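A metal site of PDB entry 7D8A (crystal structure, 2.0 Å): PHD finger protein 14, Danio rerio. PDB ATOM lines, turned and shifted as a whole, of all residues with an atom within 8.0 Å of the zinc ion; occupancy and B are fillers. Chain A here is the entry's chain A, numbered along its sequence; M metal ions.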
ATOM      1  N   GLN A  27      -7.555 -27.321  -2.339  1.00  0.00           N
ATOM      2  CA  GLN A  27      -7.833 -28.548  -3.075  1.00  0.00           C
ATOM      3  C   GLN A  27      -8.995 -29.291  -2.442  1.00  0.00           C
ATOM      4  O   GLN A  27      -9.057 -29.453  -1.222  1.00  0.00           O
ATOM      5  CB  GLN A  27      -6.605 -29.463  -3.108  1.00  0.00           C
ATOM      6  CG  GLN A  27      -6.854 -30.708  -3.935  1.00  0.00           C
ATOM      7  CD  GLN A  27      -5.591 -31.498  -4.179  1.00  0.00           C
ATOM      8  OE1 GLN A  27      -4.723 -31.569  -3.304  1.00  0.00           O
ATOM      9  NE2 GLN A  27      -5.473 -32.091  -5.359  1.00  0.00           N
ATOM     10  N   CYS A  28      -9.918 -29.748  -3.292  1.00  0.00           N
ATOM     11  CA  CYS A  28     -10.993 -30.611  -2.802  1.00  0.00           C
ATOM     12  C   CYS A  28     -10.438 -31.994  -2.469  1.00  0.00           C
ATOM     13  O   CYS A  28      -9.794 -32.641  -3.293  1.00  0.00           O
ATOM     14  CB  CYS A  28     -12.095 -30.727  -3.833  1.00  0.00           C
ATOM     15  SG  CYS A  28     -13.337 -31.906  -3.333  1.00  0.00           S
ATOM     16  N   ASP A  29     -10.723 -32.455  -1.250  1.00  0.00           N
ATOM     17  CA  ASP A  29     -10.160 -33.710  -0.780  1.00  0.00           C
ATOM     18  C   ASP A  29     -10.901 -34.941  -1.287  1.00  0.00           C
ATOM     19  O   ASP A  29     -10.552 -36.061  -0.886  1.00  0.00           O
ATOM     20  CB  ASP A  29     -10.119 -33.732   0.754  1.00  0.00           C
ATOM     21  CG  ASP A  29      -9.000 -32.861   1.318  1.00  0.00           C
ATOM     22  OD1 ASP A  29      -7.874 -32.904   0.777  1.00  0.00           O
ATOM     23  OD2 ASP A  29      -9.248 -32.151   2.309  1.00  0.00           O
ATOM     24  N   ASN A  30     -11.923 -34.792  -2.135  1.00  0.00           N
ATOM     25  CA  ASN A  30     -12.581 -35.945  -2.731  1.00  0.00           C
ATOM     26  C   ASN A  30     -12.325 -36.081  -4.224  1.00  0.00           C
ATOM     27  O   ASN A  30     -11.936 -37.151  -4.686  1.00  0.00           O
ATOM     28  CB  ASN A  30     -14.089 -35.895  -2.489  1.00  0.00           C
ATOM     29  CG  ASN A  30     -14.797 -37.088  -3.094  1.00  0.00           C
ATOM     30  OD1 ASN A  30     -14.428 -38.232  -2.841  1.00  0.00           O
ATOM     31  ND2 ASN A  30     -15.797 -36.827  -3.944  1.00  0.00           N
ATOM     32  N   CYS A  31     -12.602 -35.025  -5.001  1.00  0.00           N
ATOM     33  CA  CYS A  31     -12.396 -35.068  -6.452  1.00  0.00           C
ATOM     34  C   CYS A  31     -11.059 -34.492  -6.871  1.00  0.00           C
ATOM     35  O   CYS A  31     -10.658 -34.694  -8.027  1.00  0.00           O
ATOM     36  CB  CYS A  31     -13.520 -34.301  -7.162  1.00  0.00           C
ATOM     37  SG  CYS A  31     -13.504 -32.540  -6.865  1.00  0.00           S
ATOM     38  N   GLY A  32     -10.362 -33.781  -5.982  1.00  0.00           N
ATOM     39  CA  GLY A  32      -9.020 -33.309  -6.236  1.00  0.00           C
ATOM     40  C   GLY A  32      -8.887 -31.963  -6.906  1.00  0.00           C
ATOM     41  O   GLY A  32      -7.758 -31.475  -7.076  1.00  0.00           O
ATOM     42  N   VAL A  33      -9.995 -31.320  -7.295  1.00  0.00           N
ATOM     43  CA  VAL A  33      -9.896 -30.060  -8.005  1.00  0.00           C
ATOM     44  C   VAL A  33      -9.249 -29.005  -7.111  1.00  0.00           C
ATOM     45  O   VAL A  33      -9.400 -29.003  -5.887  1.00  0.00           O
ATOM     46  CB  VAL A  33     -11.276 -29.577  -8.517  1.00  0.00           C
ATOM     47  CG1 VAL A  33     -11.860 -30.587  -9.483  1.00  0.00           C
ATOM     48  CG2 VAL A  33     -12.214 -29.318  -7.359  1.00  0.00           C
ATOM     49  N   THR A  34      -8.482 -28.116  -7.755  1.00  0.00           N
ATOM     50  CA  THR A  34      -7.765 -27.039  -7.092  1.00  0.00           C
ATOM     51  C   THR A  34      -8.277 -25.698  -7.595  1.00  0.00           C
ATOM     52  O   THR A  34      -8.494 -25.510  -8.799  1.00  0.00           O
ATOM     53  CB  THR A  34      -6.248 -27.176  -7.345  1.00  0.00           C
ATOM     54  OG1 THR A  34      -6.015 -27.371  -8.734  1.00  0.00           O
ATOM     55  CG2 THR A  34      -5.700 -28.370  -6.573  1.00  0.00           C
ATOM     56  N   TYR A  40     -13.807 -19.031  -5.996  1.00  0.00           N
ATOM     57  CA  TYR A  40     -14.904 -19.943  -5.705  1.00  0.00           C
ATOM     58  C   TYR A  40     -15.846 -19.415  -4.636  1.00  0.00           C
ATOM     59  O   TYR A  40     -16.788 -20.115  -4.267  1.00  0.00           O
ATOM     60  CB  TYR A  40     -14.343 -21.301  -5.271  1.00  0.00           C
ATOM     61  CG  TYR A  40     -15.297 -22.476  -5.373  1.00  0.00           C
ATOM     62  CD1 TYR A  40     -15.897 -22.819  -6.576  1.00  0.00           C
ATOM     63  CD2 TYR A  40     -15.560 -23.284  -4.262  1.00  0.00           C
ATOM     64  CE1 TYR A  40     -16.756 -23.914  -6.673  1.00  0.00           C
ATOM     65  CE2 TYR A  40     -16.402 -24.371  -4.344  1.00  0.00           C
ATOM     66  CZ  TYR A  40     -17.000 -24.686  -5.549  1.00  0.00           C
ATOM     67  OH  TYR A  40     -17.842 -25.771  -5.601  1.00  0.00           O
ATOM     68  N   TRP A  61     -11.114 -29.807   3.024  1.00  0.00           N
ATOM     69  CA  TRP A  61     -12.022 -28.992   2.217  1.00  0.00           C
ATOM     70  C   TRP A  61     -12.655 -29.848   1.127  1.00  0.00           C
ATOM     71  O   TRP A  61     -12.022 -30.764   0.587  1.00  0.00           O
ATOM     72  CB  TRP A  61     -11.323 -27.794   1.564  1.00  0.00           C
ATOM     73  CG  TRP A  61     -12.300 -26.878   0.865  1.00  0.00           C
ATOM     74  CD1 TRP A  61     -13.197 -26.039   1.462  1.00  0.00           C
ATOM     75  CD2 TRP A  61     -12.503 -26.735  -0.559  1.00  0.00           C
ATOM     76  NE1 TRP A  61     -13.940 -25.379   0.502  1.00  0.00           N
ATOM     77  CE2 TRP A  61     -13.527 -25.784  -0.740  1.00  0.00           C
ATOM     78  CE3 TRP A  61     -11.905 -27.317  -1.680  1.00  0.00           C
ATOM     79  CZ2 TRP A  61     -13.981 -25.402  -2.009  1.00  0.00           C
ATOM     80  CZ3 TRP A  61     -12.359 -26.935  -2.949  1.00  0.00           C
ATOM     81  CH2 TRP A  61     -13.381 -25.987  -3.092  1.00  0.00           C
ATOM     82  N   PHE A  62     -13.912 -29.525   0.796  1.00  0.00           N
ATOM     83  CA  PHE A  62     -14.660 -30.219  -0.242  1.00  0.00           C
ATOM     84  C   PHE A  62     -15.437 -29.200  -1.068  1.00  0.00           C
ATOM     85  O   PHE A  62     -16.040 -28.271  -0.509  1.00  0.00           O
ATOM     86  CB  PHE A  62     -15.645 -31.233   0.363  1.00  0.00           C
ATOM     87  CG  PHE A  62     -14.976 -32.276   1.223  1.00  0.00           C
ATOM     88  CD1 PHE A  62     -14.274 -33.321   0.645  1.00  0.00           C
ATOM     89  CD2 PHE A  62     -15.056 -32.207   2.597  1.00  0.00           C
ATOM     90  CE1 PHE A  62     -13.669 -34.270   1.415  1.00  0.00           C
ATOM     91  CE2 PHE A  62     -14.458 -33.167   3.385  1.00  0.00           C
ATOM     92  CZ  PHE A  62     -13.759 -34.199   2.792  1.00  0.00           C
ATOM     93  N   CYS A  63     -15.421 -29.367  -2.388  1.00  0.00           N
ATOM     94  CA  CYS A  63     -16.195 -28.512  -3.278  1.00  0.00           C
ATOM     95  C   CYS A  63     -17.697 -28.777  -3.111  1.00  0.00           C
ATOM     96  O   CYS A  63     -18.108 -29.755  -2.490  1.00  0.00           O
ATOM     97  CB  CYS A  63     -15.763 -28.733  -4.729  1.00  0.00           C
ATOM     98  SG  CYS A  63     -16.378 -30.293  -5.451  1.00  0.00           S
ATOM     99  N   ASP A  64     -18.518 -27.894  -3.691  1.00  0.00           N
ATOM    100  CA  ASP A  64     -19.970 -27.997  -3.517  1.00  0.00           C
ATOM    101  C   ASP A  64     -20.530 -29.279  -4.131  1.00  0.00           C
ATOM    102  O   ASP A  64     -21.489 -29.854  -3.608  1.00  0.00           O
ATOM    103  CB  ASP A  64     -20.670 -26.783  -4.123  1.00  0.00           C
ATOM    104  CG  ASP A  64     -20.361 -25.479  -3.382  1.00  0.00           C
ATOM    105  OD1 ASP A  64     -19.667 -25.516  -2.349  1.00  0.00           O
ATOM    106  OD2 ASP A  64     -20.813 -24.416  -3.847  1.00  0.00           O
ATOM    107  N   ALA A  65     -19.949 -29.738  -5.248  1.00  0.00           N
ATOM    108  CA  ALA A  65     -20.466 -30.939  -5.884  1.00  0.00           C
ATOM    109  C   ALA A  65     -20.209 -32.177  -5.017  1.00  0.00           C
ATOM    110  O   ALA A  65     -21.077 -33.050  -4.903  1.00  0.00           O
ATOM    111  CB  ALA A  65     -19.847 -31.123  -7.271  1.00  0.00           C
ATOM    112  N   CYS A  66     -19.040 -32.242  -4.380  1.00  0.00           N
ATOM    113  CA  CYS A  66     -18.752 -33.365  -3.489  1.00  0.00           C
ATOM    114  C   CYS A  66     -19.578 -33.286  -2.207  1.00  0.00           C
ATOM    115  O   CYS A  66     -20.007 -34.315  -1.682  1.00  0.00           O
ATOM    116  CB  CYS A  66     -17.265 -33.421  -3.187  1.00  0.00           C
ATOM    117  SG  CYS A  66     -16.305 -33.925  -4.635  1.00  0.00           S
ATOM    118  N   LYS A  67     -19.817 -32.077  -1.690  1.00  0.00           N
ATOM    119  CA  LYS A  67     -20.687 -31.935  -0.518  1.00  0.00           C
ATOM    120  C   LYS A  67     -22.064 -32.557  -0.767  1.00  0.00           C
ATOM    121  O   LYS A  67     -22.698 -33.047   0.167  1.00  0.00           O
ATOM    122  CB  LYS A  67     -20.871 -30.473  -0.131  1.00  0.00           C
ATOM    123  CG  LYS A  67     -19.690 -29.819   0.579  1.00  0.00           C
ATOM    124  CD  LYS A  67     -20.156 -28.560   1.311  1.00  0.00           C
ATOM    125  CE  LYS A  67     -19.045 -27.520   1.442  1.00  0.00           C
ATOM    126  NZ  LYS A  67     -17.875 -27.997   2.233  1.00  0.00           N
ATOM    127  N   VAL A  70     -22.428 -35.617  -5.760  1.00  0.00           N
ATOM    128  CA  VAL A  70     -22.630 -35.746  -7.193  1.00  0.00           C
ATOM    129  C   VAL A  70     -21.317 -35.471  -7.925  1.00  0.00           C
ATOM    130  O   VAL A  70     -20.443 -34.750  -7.441  1.00  0.00           O
ATOM    131  CB  VAL A  70     -23.748 -34.817  -7.722  1.00  0.00           C
ATOM    132  CG1 VAL A  70     -25.076 -35.150  -7.076  1.00  0.00           C
ATOM    133  CG2 VAL A  70     -23.394 -33.350  -7.501  1.00  0.00           C
ATOM    134  N   PRO A  72     -21.101 -33.960 -11.287  1.00  0.00           N
ATOM    135  CA  PRO A  72     -22.151 -33.443 -12.170  1.00  0.00           C
ATOM    136  C   PRO A  72     -21.658 -33.201 -13.583  1.00  0.00           C
ATOM    137  O   PRO A  72     -20.462 -33.253 -13.892  1.00  0.00           O
ATOM    138  CB  PRO A  72     -22.542 -32.122 -11.485  1.00  0.00           C
ATOM    139  CG  PRO A  72     -21.266 -31.649 -10.878  1.00  0.00           C
ATOM    140  CD  PRO A  72     -20.517 -32.899 -10.453  1.00  0.00           C
ATOM    141  N   GLY A  82     -13.013 -29.862 -13.838  1.00  0.00           N
ATOM    142  CA  GLY A  82     -13.139 -28.528 -13.281  1.00  0.00           C
ATOM    143  C   GLY A  82     -14.105 -28.515 -12.101  1.00  0.00           C
ATOM    144  O   GLY A  82     -14.483 -29.559 -11.548  1.00  0.00           O
ATOM    145  N   ILE A  83     -14.492 -27.302 -11.704  1.00  0.00           N
ATOM    146  CA  ILE A  83     -15.225 -27.125 -10.456  1.00  0.00           C
ATOM    147  C   ILE A  83     -16.572 -26.457 -10.745  1.00  0.00           C
ATOM    148  O   ILE A  83     -16.675 -25.620 -11.665  1.00  0.00           O
ATOM    149  CB  ILE A  83     -14.368 -26.341  -9.435  1.00  0.00           C
ATOM    150  CG1 ILE A  83     -14.860 -26.617  -8.012  1.00  0.00           C
ATOM    151  CG2 ILE A  83     -14.272 -24.866  -9.793  1.00  0.00           C
ATOM    152  CD1 ILE A  83     -13.966 -26.037  -6.950  1.00  0.00           C
ATOM    153  N   PHE A  84     -17.591 -26.862  -9.988  1.00  0.00           N
ATOM    154  CA  PHE A  84     -18.999 -26.575 -10.284  1.00  0.00           C
ATOM    155  C   PHE A  84     -19.682 -25.829  -9.146  1.00  0.00           C
ATOM    156  O   PHE A  84     -19.264 -25.905  -7.979  1.00  0.00           O
ATOM    157  CB  PHE A  84     -19.791 -27.874 -10.526  1.00  0.00           C
ATOM    158  CG  PHE A  84     -19.375 -28.640 -11.747  1.00  0.00           C
ATOM    159  CD1 PHE A  84     -20.079 -28.511 -12.927  1.00  0.00           C
ATOM    160  CD2 PHE A  84     -18.274 -29.483 -11.709  1.00  0.00           C
ATOM    161  CE1 PHE A  84     -19.702 -29.223 -14.063  1.00  0.00           C
ATOM    162  CE2 PHE A  84     -17.885 -30.202 -12.841  1.00  0.00           C
ATOM    163  CZ  PHE A  84     -18.608 -30.071 -14.015  1.00  0.00           C
HETATM  164 ZN    ZN M   1     -14.840 -32.014  -5.162  1.00  0.00          ZN
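SG of Cys 31 sits close to N of Val 33, 3.7 Å away. The side-chain sulfur (SG) of Cys 63 lies close to the backbone NH (N) of Ala 65, 3.6 Å away. N of Cys 28 sits at hydrogen-bond distance from O of Val 33 (2.7 Å). SG of Cys 28 lies close to N of Asn 30 (3.4 Å). SG of Cys 66 sits close to ND2 of Asn 30.
The nearest printed residue that does not touch the zinc ion is Val 33 (4.4 Å).
SG of Cys 31 binds the zinc ion. The side-chain sulfur (SG) of Cys 63 is bound to the zinc ion, at 2.3 Å. The side-chain sulfur (SG) of Cys 28 binds the zinc ion (2.4 Å). The zinc ion is bound by the side-chain sulfur (SG) of Cys 66 (2.5 Å). The zinc ion has four donor atoms within binding distance.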
